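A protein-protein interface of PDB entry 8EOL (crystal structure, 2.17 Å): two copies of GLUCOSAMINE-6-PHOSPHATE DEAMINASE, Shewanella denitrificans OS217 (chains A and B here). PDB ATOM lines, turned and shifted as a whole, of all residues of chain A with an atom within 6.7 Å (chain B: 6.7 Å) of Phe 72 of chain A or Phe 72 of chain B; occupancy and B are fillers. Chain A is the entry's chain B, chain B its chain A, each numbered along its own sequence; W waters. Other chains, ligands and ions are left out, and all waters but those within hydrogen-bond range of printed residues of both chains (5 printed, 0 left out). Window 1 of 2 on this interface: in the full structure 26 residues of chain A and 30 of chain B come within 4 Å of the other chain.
Water W1 lies within hydrogen-bond range of OE2 of Glu 64 of chain B (2.5 Å), NZ of Lys 60 of chain B (2.8 Å) and SD of Met 45 of chain A (3.5 Å). Water W5 lies within hydrogen-bond range of the side-chain carboxylate of Glu 64 of chain B and the backbone NH of Ala 75 of chain A. Water W2 lies within hydrogen-bond range of OE2 of Glu 64 of chain A (2.6 Å), NZ of Lys 60 of chain A (2.9 Å) and SD of Met 45 of chain B (3.4 Å). Water W3 bridges the side-chain amino group (NZ) of Lys 60 of chain B (2.7 Å) and the backbone carbonyl oxygen (O) of Ala 73 of chain A (2.8 Å). Water W4 lies within hydrogen-bond range of the backbone carbonyl oxygen of Ala 73 of chain B (2.8 Å) and the side-chain amino group of Lys 60 of chain A (3.1 Å).
Of the printed residues of chain B, Lys 60 of chain A touches Ala 73 (3.2 Å). Of the printed residues of chain B, Glu 64 of chain A touches Leu 86 (3.6 Å). Of the printed residues of chain B, Phe 72 of chain A touches Pro 70 and Phe 72. Of the printed residues of chain B, Ala 75 of chain A touches Lys 60. Met 45 of chain B touches none of the printed residues of chain A. Printed residues of chain A within 4 Å of Glu 64 of chain B: Leu 86. Of chain A, only Pro 70 (3.7 Å) and Phe 72 (3.2 Å) come within 4 Å of Phe 72 of chain B. Printed residues of chain A within 4 Å of Leu 86 of chain B: Glu 64 (3.6 Å).
Among the printed residues, merely in contact across the chains: Phe 72 of chain A with Phe 72 of chain B, Ala 75 of chain A with Lys 60 of chain B, Glu 64 of chain A with Leu 86 of chain B, Pro 70 of chain A with Phe 72 of chain B, Leu 86 of chain A with Glu 64 of chain B, Phe 72 of chain A with Pro 70 of chain B and Pro 70 of chain A with Leu 88 of chain B.
O of Ala 73 of chain B lies within hydrogen-bond range of NZ of Lys 60 of chain A. NZ of Lys 60 of chain B sits at hydrogen-bond distance from O of Ala 73 of chain A.
Of the 17 printed residues of chain A, 7 touch a printed residue of chain B. Hydrophobic or aromatic side chains of chain A within 4 Å of the printed part of chain B: Pro 70, Phe 72, Ala 75 and Leu 86. Among the printed residues, no Asp or Glu carboxylate lies within 4 Å of a Lys or Arg side-chain nitrogen of the other chain.
O of Thr 71 of chain A is in hydrogen-bond range of NZ of Lys 60 of chain A, at 2.7 Å. The backbone NH of Ile 46 of chain A sits at hydrogen-bond distance from the backbone carbonyl oxygen of Phe 72 of chain A (2.7 Å). The backbone NH (N) of Val 44 of chain A sits at hydrogen-bond distance from the backbone carbonyl oxygen (O) of Pro 70 of chain A, at 2.9 Å. The side-chain carboxylate (OE2) of Glu 64 of chain B is in hydrogen-bond range of the backbone NH (N) of Thr 71 of chain B (2.9 Å). NZ of Lys 60 of chain B is in hydrogen-bond range of O of Thr 71 of chain B (2.7 Å). The side-chain amino group (NZ) of Lys 60 of chain A lies within salt-bridge range of the side-chain carboxylate (OE2) of Glu 64 of chain A, at 2.8 Å.
Lys 60 of chain A touches Ala 73 of chain B, and with the chains exchanged Ala 73 of chain A touches Lys 60 of chain B. Glu 64 of chain A touches Leu 86 of chain B, and with the chains exchanged Leu 86 of chain A touches Glu 64 of chain B. Pro 70 of chain A touches Phe 72 of chain B, and with the chains exchanged Phe 72 of chain A touches Pro 70 of chain B. Phe 72 of chain A touches its own counterpart, Phe 72 of chain B.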
ATOM      1  N   PHE A  43     -22.749  11.060  21.932  1.00  0.00           N
ATOM      2  CA  PHE A  43     -22.803  11.260  20.487  1.00  0.00           C
ATOM      3  C   PHE A  43     -21.523  11.978  20.107  1.00  0.00           C
ATOM      4  O   PHE A  43     -20.828  12.515  20.976  1.00  0.00           O
ATOM      5  CB  PHE A  43     -24.031  12.074  20.050  1.00  0.00           C
ATOM      6  CG  PHE A  43     -24.140  13.389  20.743  1.00  0.00           C
ATOM      7  CD1 PHE A  43     -23.349  14.465  20.342  1.00  0.00           C
ATOM      8  CD2 PHE A  43     -25.029  13.562  21.794  1.00  0.00           C
ATOM      9  CE1 PHE A  43     -23.435  15.689  20.984  1.00  0.00           C
ATOM     10  CE2 PHE A  43     -25.125  14.809  22.468  1.00  0.00           C
ATOM     11  CZ  PHE A  43     -24.333  15.870  22.054  1.00  0.00           C
ATOM     12  N   VAL A  44     -21.207  11.963  18.811  1.00  0.00           N
ATOM     13  CA  VAL A  44     -20.044  12.648  18.254  1.00  0.00           C
ATOM     14  C   VAL A  44     -20.545  13.630  17.208  1.00  0.00           C
ATOM     15  O   VAL A  44     -21.175  13.231  16.215  1.00  0.00           O
ATOM     16  CB  VAL A  44     -19.031  11.680  17.631  1.00  0.00           C
ATOM     17  CG1 VAL A  44     -17.759  12.459  17.150  1.00  0.00           C
ATOM     18  CG2 VAL A  44     -18.674  10.536  18.627  1.00  0.00           C
ATOM     19  N   MET A  45     -20.264  14.908  17.425  1.00  0.00           N
ATOM     20  CA  MET A  45     -20.604  15.935  16.461  1.00  0.00           C
ATOM     21  C   MET A  45     -19.317  16.435  15.835  1.00  0.00           C
ATOM     22  O   MET A  45     -18.373  16.794  16.543  1.00  0.00           O
ATOM     23  CB  MET A  45     -21.389  17.081  17.102  1.00  0.00           C
ATOM     24  CG  MET A  45     -21.687  18.230  16.139  1.00  0.00           C
ATOM     25  SD  MET A  45     -22.807  19.463  16.894  1.00  0.00           S
ATOM     26  CE  MET A  45     -21.599  20.608  17.585  1.00  0.00           C
ATOM     27  N   ILE A  46     -19.280  16.449  14.507  1.00  0.00           N
ATOM     28  CA  ILE A  46     -18.109  16.891  13.771  1.00  0.00           C
ATOM     29  C   ILE A  46     -18.325  18.332  13.302  1.00  0.00           C
ATOM     30  O   ILE A  46     -19.301  18.627  12.597  1.00  0.00           O
ATOM     31  CB  ILE A  46     -17.837  15.978  12.569  1.00  0.00           C
ATOM     32  CG1 ILE A  46     -17.878  14.494  12.942  1.00  0.00           C
ATOM     33  CG2 ILE A  46     -16.565  16.411  11.863  1.00  0.00           C
ATOM     34  CD1 ILE A  46     -16.875  14.057  13.949  1.00  0.00           C
ATOM     35  N   VAL A  47     -17.384  19.208  13.647  1.00  0.00           N
ATOM     36  CA  VAL A  47     -17.345  20.604  13.208  1.00  0.00           C
ATOM     37  C   VAL A  47     -16.247  20.705  12.158  1.00  0.00           C
ATOM     38  O   VAL A  47     -15.099  20.320  12.417  1.00  0.00           O
ATOM     39  CB  VAL A  47     -17.047  21.563  14.381  1.00  0.00           C
ATOM     40  CG1 VAL A  47     -16.808  22.991  13.889  1.00  0.00           C
ATOM     41  CG2 VAL A  47     -18.100  21.507  15.456  1.00  0.00           C
ATOM     42  N   GLY A  56     -15.693  14.301   7.840  1.00  0.00           N
ATOM     43  CA  GLY A  56     -16.780  14.078   8.785  1.00  0.00           C
ATOM     44  C   GLY A  56     -17.690  12.934   8.389  1.00  0.00           C
ATOM     45  O   GLY A  56     -18.181  12.198   9.245  1.00  0.00           O
ATOM     46  N   LYS A  60     -18.296   9.592  10.546  1.00  0.00           N
ATOM     47  CA  LYS A  60     -19.611   9.066  10.895  1.00  0.00           C
ATOM     48  C   LYS A  60     -19.626   7.549  10.809  1.00  0.00           C
ATOM     49  O   LYS A  60     -20.009   6.872  11.767  1.00  0.00           O
ATOM     50  CB  LYS A  60     -20.708   9.667  10.006  1.00  0.00           C
ATOM     51  CG  LYS A  60     -22.122   9.058  10.294  1.00  0.00           C
ATOM     52  CD  LYS A  60     -23.234   9.805   9.545  1.00  0.00           C
ATOM     53  CE  LYS A  60     -24.580   9.161   9.872  1.00  0.00           C
ATOM     54  NZ  LYS A  60     -25.067   9.557  11.217  1.00  0.00           N
ATOM     55  N   GLU A  64     -19.749   5.279  14.364  1.00  0.00           N
ATOM     56  CA  GLU A  64     -20.976   4.501  14.518  1.00  0.00           C
ATOM     57  C   GLU A  64     -20.672   3.011  14.394  1.00  0.00           C
ATOM     58  O   GLU A  64     -21.196   2.186  15.156  1.00  0.00           O
ATOM     59  CB  GLU A  64     -22.019   4.930  13.480  1.00  0.00           C
ATOM     60  CG  GLU A  64     -22.517   6.351  13.749  1.00  0.00           C
ATOM     61  CD  GLU A  64     -23.775   6.748  12.952  1.00  0.00           C
ATOM     62  OE1 GLU A  64     -24.167   6.032  11.996  1.00  0.00           O
ATOM     63  OE2 GLU A  64     -24.367   7.790  13.298  1.00  0.00           O
ATOM     64  N   ILE A  69     -21.519   4.812  18.536  1.00  0.00           N
ATOM     65  CA  ILE A  69     -21.912   6.126  19.035  1.00  0.00           C
ATOM     66  C   ILE A  69     -22.450   6.945  17.864  1.00  0.00           C
ATOM     67  O   ILE A  69     -21.707   7.181  16.912  1.00  0.00           O
ATOM     68  CB  ILE A  69     -20.736   6.864  19.689  1.00  0.00           C
ATOM     69  CG1 ILE A  69     -20.158   6.037  20.850  1.00  0.00           C
ATOM     70  CG2 ILE A  69     -21.199   8.271  20.076  1.00  0.00           C
ATOM     71  CD1 ILE A  69     -21.125   5.839  21.968  1.00  0.00           C
ATOM     72  N   PRO A  70     -23.697   7.424  17.918  1.00  0.00           N
ATOM     73  CA  PRO A  70     -24.243   8.233  16.823  1.00  0.00           C
ATOM     74  C   PRO A  70     -23.342   9.419  16.550  1.00  0.00           C
ATOM     75  O   PRO A  70     -23.013  10.172  17.460  1.00  0.00           O
ATOM     76  CB  PRO A  70     -25.605   8.714  17.360  1.00  0.00           C
ATOM     77  CG  PRO A  70     -25.753   8.181  18.686  1.00  0.00           C
ATOM     78  CD  PRO A  70     -24.620   7.294  19.053  1.00  0.00           C
ATOM     79  N   THR A  71     -23.011   9.620  15.283  1.00  0.00           N
ATOM     80  CA  THR A  71     -22.083  10.645  14.839  1.00  0.00           C
ATOM     81  C   THR A  71     -22.706  11.470  13.706  1.00  0.00           C
ATOM     82  O   THR A  71     -23.434  10.925  12.879  1.00  0.00           O
ATOM     83  CB  THR A  71     -20.794   9.962  14.386  1.00  0.00           C
ATOM     84  OG1 THR A  71     -20.282   9.175  15.474  1.00  0.00           O
ATOM     85  CG2 THR A  71     -19.739  10.971  13.915  1.00  0.00           C
ATOM     86  N   PHE A  72     -22.431  12.785  13.667  1.00  0.00           N
ATOM     87  CA  PHE A  72     -23.079  13.645  12.678  1.00  0.00           C
ATOM     88  C   PHE A  72     -22.320  14.971  12.555  1.00  0.00           C
ATOM     89  O   PHE A  72     -21.480  15.325  13.395  1.00  0.00           O
ATOM     90  CB  PHE A  72     -24.546  13.877  13.058  1.00  0.00           C
ATOM     91  CG  PHE A  72     -24.708  14.440  14.439  1.00  0.00           C
ATOM     92  CD1 PHE A  72     -24.738  13.618  15.532  1.00  0.00           C
ATOM     93  CD2 PHE A  72     -24.753  15.813  14.634  1.00  0.00           C
ATOM     94  CE1 PHE A  72     -24.828  14.168  16.809  1.00  0.00           C
ATOM     95  CE2 PHE A  72     -24.835  16.359  15.901  1.00  0.00           C
ATOM     96  CZ  PHE A  72     -24.866  15.547  16.984  1.00  0.00           C
ATOM     97  N   ALA A  73     -22.633  15.714  11.494  1.00  0.00           N
ATOM     98  CA  ALA A  73     -21.968  16.990  11.228  1.00  0.00           C
ATOM     99  C   ALA A  73     -22.778  18.141  11.818  1.00  0.00           C
ATOM    100  O   ALA A  73     -24.014  18.150  11.757  1.00  0.00           O
ATOM    101  CB  ALA A  73     -21.767  17.203   9.723  1.00  0.00           C
ATOM    102  N   ALA A  74     -22.070  19.110  12.404  1.00  0.00           N
ATOM    103  CA  ALA A  74     -22.716  20.322  12.889  1.00  0.00           C
ATOM    104  C   ALA A  74     -23.255  21.134  11.711  1.00  0.00           C
ATOM    105  O   ALA A  74     -22.769  21.021  10.579  1.00  0.00           O
ATOM    106  CB  ALA A  74     -21.739  21.160  13.692  1.00  0.00           C
ATOM    107  N   ALA A  75     -24.310  21.916  11.975  1.00  0.00           N
ATOM    108  CA  ALA A  75     -24.799  22.925  11.039  1.00  0.00           C
ATOM    109  C   ALA A  75     -24.349  24.293  11.535  1.00  0.00           C
ATOM    110  O   ALA A  75     -24.989  24.864  12.434  1.00  0.00           O
ATOM    111  CB  ALA A  75     -26.325  22.875  10.914  1.00  0.00           C
ATOM    112  N   LEU A  86     -26.634  24.831  21.128  1.00  0.00           N
ATOM    113  CA  LEU A  86     -27.130  23.475  21.277  1.00  0.00           C
ATOM    114  C   LEU A  86     -26.778  22.913  22.645  1.00  0.00           C
ATOM    115  O   LEU A  86     -25.714  23.191  23.201  1.00  0.00           O
ATOM    116  CB  LEU A  86     -26.557  22.536  20.216  1.00  0.00           C
ATOM    117  CG  LEU A  86     -26.903  22.668  18.731  1.00  0.00           C
ATOM    118  CD1 LEU A  86     -26.111  21.643  17.966  1.00  0.00           C
ATOM    119  CD2 LEU A  86     -28.377  22.430  18.518  1.00  0.00           C
ATOM    120  N   LEU A  88     -25.182  20.261  24.249  1.00  0.00           N
ATOM    121  CA  LEU A  88     -24.175  19.285  23.877  1.00  0.00           C
ATOM    122  C   LEU A  88     -23.573  18.596  25.091  1.00  0.00           C
ATOM    123  O   LEU A  88     -22.571  17.887  24.953  1.00  0.00           O
ATOM    124  CB  LEU A  88     -23.075  19.957  23.054  1.00  0.00           C
ATOM    125  CG  LEU A  88     -23.524  20.631  21.769  1.00  0.00           C
ATOM    126  CD1 LEU A  88     -22.427  21.503  21.160  1.00  0.00           C
ATOM    127  CD2 LEU A  88     -23.930  19.553  20.783  1.00  0.00           C
ATOM    128  N   PHE B  43     -31.058  14.022  21.768  1.00  0.00           N
ATOM    129  CA  PHE B  43     -30.795  14.255  20.348  1.00  0.00           C
ATOM    130  C   PHE B  43     -31.983  13.687  19.578  1.00  0.00           C
ATOM    131  O   PHE B  43     -32.763  12.892  20.111  1.00  0.00           O
ATOM    132  CB  PHE B  43     -29.483  13.615  19.871  1.00  0.00           C
ATOM    133  CG  PHE B  43     -29.404  12.153  20.140  1.00  0.00           C
ATOM    134  CD1 PHE B  43     -30.063  11.242  19.324  1.00  0.00           C
ATOM    135  CD2 PHE B  43     -28.705  11.684  21.233  1.00  0.00           C
ATOM    136  CE1 PHE B  43     -30.010   9.887  19.598  1.00  0.00           C
ATOM    137  CE2 PHE B  43     -28.642  10.307  21.510  1.00  0.00           C
ATOM    138  CZ  PHE B  43     -29.300   9.422  20.698  1.00  0.00           C
ATOM    139  N   VAL B  44     -32.092  14.079  18.312  1.00  0.00           N
ATOM    140  CA  VAL B  44     -33.133  13.602  17.410  1.00  0.00           C
ATOM    141  C   VAL B  44     -32.438  12.985  16.199  1.00  0.00           C
ATOM    142  O   VAL B  44     -31.640  13.653  15.526  1.00  0.00           O
ATOM    143  CB  VAL B  44     -34.084  14.738  16.984  1.00  0.00           C
ATOM    144  CG1 VAL B  44     -35.262  14.168  16.184  1.00  0.00           C
ATOM    145  CG2 VAL B  44     -34.601  15.485  18.207  1.00  0.00           C
ATOM    146  N   MET B  45     -32.711  11.717  15.932  1.00  0.00           N
ATOM    147  CA  MET B  45     -32.163  11.062  14.759  1.00  0.00           C
ATOM    148  C   MET B  45     -33.297  10.825  13.781  1.00  0.00           C
ATOM    149  O   MET B  45     -34.344  10.297  14.162  1.00  0.00           O
ATOM    150  CB  MET B  45     -31.468   9.746  15.125  1.00  0.00           C
ATOM    151  CG  MET B  45     -30.988   8.950  13.947  1.00  0.00           C
ATOM    152  SD  MET B  45     -29.905   7.556  14.432  1.00  0.00           S
ATOM    153  CE  MET B  45     -31.173   6.292  14.440  1.00  0.00           C
ATOM    154  N   ILE B  46     -33.097  11.226  12.535  1.00  0.00           N
ATOM    155  CA  ILE B  46     -34.102  11.068  11.493  1.00  0.00           C
ATOM    156  C   ILE B  46     -33.754   9.839  10.669  1.00  0.00           C
ATOM    157  O   ILE B  46     -32.650   9.739  10.116  1.00  0.00           O
ATOM    158  CB  ILE B  46     -34.180  12.309  10.586  1.00  0.00           C
ATOM    159  CG1 ILE B  46     -34.279  13.605  11.414  1.00  0.00           C
ATOM    160  CG2 ILE B  46     -35.320  12.125   9.544  1.00  0.00           C
ATOM    161  CD1 ILE B  46     -35.479  13.702  12.316  1.00  0.00           C
ATOM    162  N   VAL B  47     -34.707   8.924  10.567  1.00  0.00           N
ATOM    163  CA  VAL B  47     -34.594   7.710   9.771  1.00  0.00           C
ATOM    164  C   VAL B  47     -35.457   7.878   8.531  1.00  0.00           C
ATOM    165  O   VAL B  47     -36.632   8.245   8.634  1.00  0.00           O
ATOM    166  CB  VAL B  47     -35.045   6.466  10.562  1.00  0.00           C
ATOM    167  CG1 VAL B  47     -35.164   5.262   9.621  1.00  0.00           C
ATOM    168  CG2 VAL B  47     -34.099   6.186  11.762  1.00  0.00           C
ATOM    169  N   GLY B  56     -35.140  15.139   6.481  1.00  0.00           N
ATOM    170  CA  GLY B  56     -34.225  15.187   7.613  1.00  0.00           C
ATOM    171  C   GLY B  56     -33.423  16.473   7.718  1.00  0.00           C
ATOM    172  O   GLY B  56     -33.195  16.985   8.816  1.00  0.00           O
ATOM    173  N   ALA B  59     -35.747  18.888   9.166  1.00  0.00           N
ATOM    174  CA  ALA B  59     -35.908  18.565  10.589  1.00  0.00           C
ATOM    175  C   ALA B  59     -34.690  19.014  11.403  1.00  0.00           C
ATOM    176  O   ALA B  59     -34.836  19.505  12.528  1.00  0.00           O
ATOM    177  CB  ALA B  59     -36.175  17.065  10.790  1.00  0.00           C
ATOM    178  N   LYS B  60     -33.488  18.918  10.830  1.00  0.00           N
ATOM    179  CA  LYS B  60     -32.307  19.352  11.576  1.00  0.00           C
ATOM    180  C   LYS B  60     -32.399  20.839  11.941  1.00  0.00           C
ATOM    181  O   LYS B  60     -32.318  21.200  13.122  1.00  0.00           O
ATOM    182  CB  LYS B  60     -31.031  19.048  10.782  1.00  0.00           C
ATOM    183  CG  LYS B  60     -29.744  19.504  11.479  1.00  0.00           C
ATOM    184  CD  LYS B  60     -28.495  19.001  10.712  1.00  0.00           C
ATOM    185  CE  LYS B  60     -27.201  19.443  11.423  1.00  0.00           C
ATOM    186  NZ  LYS B  60     -26.861  18.594  12.645  1.00  0.00           N
ATOM    187  N   GLU B  64     -33.019  21.846  15.955  1.00  0.00           N
ATOM    188  CA  GLU B  64     -31.868  22.525  16.553  1.00  0.00           C
ATOM    189  C   GLU B  64     -32.192  23.987  16.881  1.00  0.00           C
ATOM    190  O   GLU B  64     -31.830  24.488  17.954  1.00  0.00           O
ATOM    191  CB  GLU B  64     -30.651  22.402  15.616  1.00  0.00           C
ATOM    192  CG  GLU B  64     -30.150  20.941  15.546  1.00  0.00           C
ATOM    193  CD  GLU B  64     -28.746  20.783  14.989  1.00  0.00           C
ATOM    194  OE1 GLU B  64     -28.163  21.772  14.460  1.00  0.00           O
ATOM    195  OE2 GLU B  64     -28.222  19.647  15.079  1.00  0.00           O
ATOM    196  N   ILE B  69     -31.862  21.033  20.363  1.00  0.00           N
ATOM    197  CA  ILE B  69     -31.556  19.610  20.488  1.00  0.00           C
ATOM    198  C   ILE B  69     -30.778  19.177  19.247  1.00  0.00           C
ATOM    199  O   ILE B  69     -31.319  19.254  18.131  1.00  0.00           O
ATOM    200  CB  ILE B  69     -32.823  18.755  20.655  1.00  0.00           C
ATOM    201  CG1 ILE B  69     -33.613  19.153  21.903  1.00  0.00           C
ATOM    202  CG2 ILE B  69     -32.426  17.281  20.713  1.00  0.00           C
ATOM    203  CD1 ILE B  69     -32.838  18.847  23.184  1.00  0.00           C
ATOM    204  N   PRO B  70     -29.556  18.662  19.396  1.00  0.00           N
ATOM    205  CA  PRO B  70     -28.804  18.183  18.228  1.00  0.00           C
ATOM    206  C   PRO B  70     -29.631  17.180  17.440  1.00  0.00           C
ATOM    207  O   PRO B  70     -30.205  16.237  18.011  1.00  0.00           O
ATOM    208  CB  PRO B  70     -27.543  17.524  18.831  1.00  0.00           C
ATOM    209  CG  PRO B  70     -27.609  17.707  20.296  1.00  0.00           C
ATOM    210  CD  PRO B  70     -28.828  18.490  20.672  1.00  0.00           C
ATOM    211  N   THR B  71     -29.720  17.405  16.114  1.00  0.00           N
ATOM    212  CA  THR B  71     -30.535  16.581  15.220  1.00  0.00           C
ATOM    213  C   THR B  71     -29.733  16.215  13.978  1.00  0.00           C
ATOM    214  O   THR B  71     -28.970  17.037  13.469  1.00  0.00           O
ATOM    215  CB  THR B  71     -31.788  17.306  14.771  1.00  0.00           C
ATOM    216  OG1 THR B  71     -32.509  17.744  15.918  1.00  0.00           O
ATOM    217  CG2 THR B  71     -32.685  16.418  13.862  1.00  0.00           C
ATOM    218  N   PHE B  72     -29.947  15.004  13.468  1.00  0.00           N
ATOM    219  CA  PHE B  72     -29.124  14.488  12.389  1.00  0.00           C
ATOM    220  C   PHE B  72     -29.819  13.300  11.755  1.00  0.00           C
ATOM    221  O   PHE B  72     -30.759  12.731  12.315  1.00  0.00           O
ATOM    222  CB  PHE B  72     -27.764  14.070  12.915  1.00  0.00           C
ATOM    223  CG  PHE B  72     -27.842  13.099  14.089  1.00  0.00           C
ATOM    224  CD1 PHE B  72     -28.020  13.571  15.381  1.00  0.00           C
ATOM    225  CD2 PHE B  72     -27.728  11.728  13.899  1.00  0.00           C
ATOM    226  CE1 PHE B  72     -28.081  12.693  16.482  1.00  0.00           C
ATOM    227  CE2 PHE B  72     -27.798  10.840  14.989  1.00  0.00           C
ATOM    228  CZ  PHE B  72     -27.969  11.327  16.285  1.00  0.00           C
ATOM    229  N   ALA B  73     -29.336  12.930  10.570  1.00  0.00           N
ATOM    230  CA  ALA B  73     -29.897  11.823   9.801  1.00  0.00           C
ATOM    231  C   ALA B  73     -29.088  10.552  10.033  1.00  0.00           C
ATOM    232  O   ALA B  73     -27.850  10.583  10.079  1.00  0.00           O
ATOM    233  CB  ALA B  73     -29.927  12.152   8.294  1.00  0.00           C
ATOM    234  N   ALA B  74     -29.799   9.432  10.154  1.00  0.00           N
ATOM    235  CA  ALA B  74     -29.175   8.118  10.170  1.00  0.00           C
ATOM    236  C   ALA B  74     -28.554   7.806   8.805  1.00  0.00           C
ATOM    237  O   ALA B  74     -29.019   8.273   7.761  1.00  0.00           O
ATOM    238  CB  ALA B  74     -30.219   7.049  10.521  1.00  0.00           C
ATOM    239  N   LEU B  86     -26.802   1.247  17.314  1.00  0.00           N
ATOM    240  CA  LEU B  86     -26.221   2.436  17.902  1.00  0.00           C
ATOM    241  C   LEU B  86     -26.748   2.555  19.322  1.00  0.00           C
ATOM    242  O   LEU B  86     -27.853   2.099  19.620  1.00  0.00           O
ATOM    243  CB  LEU B  86     -26.630   3.673  17.098  1.00  0.00           C
ATOM    244  CG  LEU B  86     -26.142   3.743  15.656  1.00  0.00           C
ATOM    245  CD1 LEU B  86     -26.728   4.979  14.912  1.00  0.00           C
ATOM    246  CD2 LEU B  86     -24.641   3.788  15.654  1.00  0.00           C
ATOM    247  N   LEU B  88     -28.646   4.590  21.457  1.00  0.00           N
ATOM    248  CA  LEU B  88     -29.651   5.630  21.261  1.00  0.00           C
ATOM    249  C   LEU B  88     -30.537   5.841  22.486  1.00  0.00           C
ATOM    250  O   LEU B  88     -31.544   6.555  22.392  1.00  0.00           O
ATOM    251  CB  LEU B  88     -30.522   5.304  20.048  1.00  0.00           C
ATOM    252  CG  LEU B  88     -29.815   5.110  18.694  1.00  0.00           C
ATOM    253  CD1 LEU B  88     -30.809   4.580  17.658  1.00  0.00           C
ATOM    254  CD2 LEU B  88     -29.195   6.399  18.246  1.00  0.00           C
HETATM  255  O   HOH W   1     -25.677  19.718  14.981  1.00  0.00           O
HETATM  256  O   HOH W   2     -26.949   8.162  12.918  1.00  0.00           O
HETATM  257  O   HOH W   3     -26.185  16.548  10.943  1.00  0.00           O
HETATM  258  O   HOH W   4     -25.634  12.322  10.029  1.00  0.00           O
HETATM  259  O   HOH W   5     -25.554  22.091  14.325  1.00  0.00           O
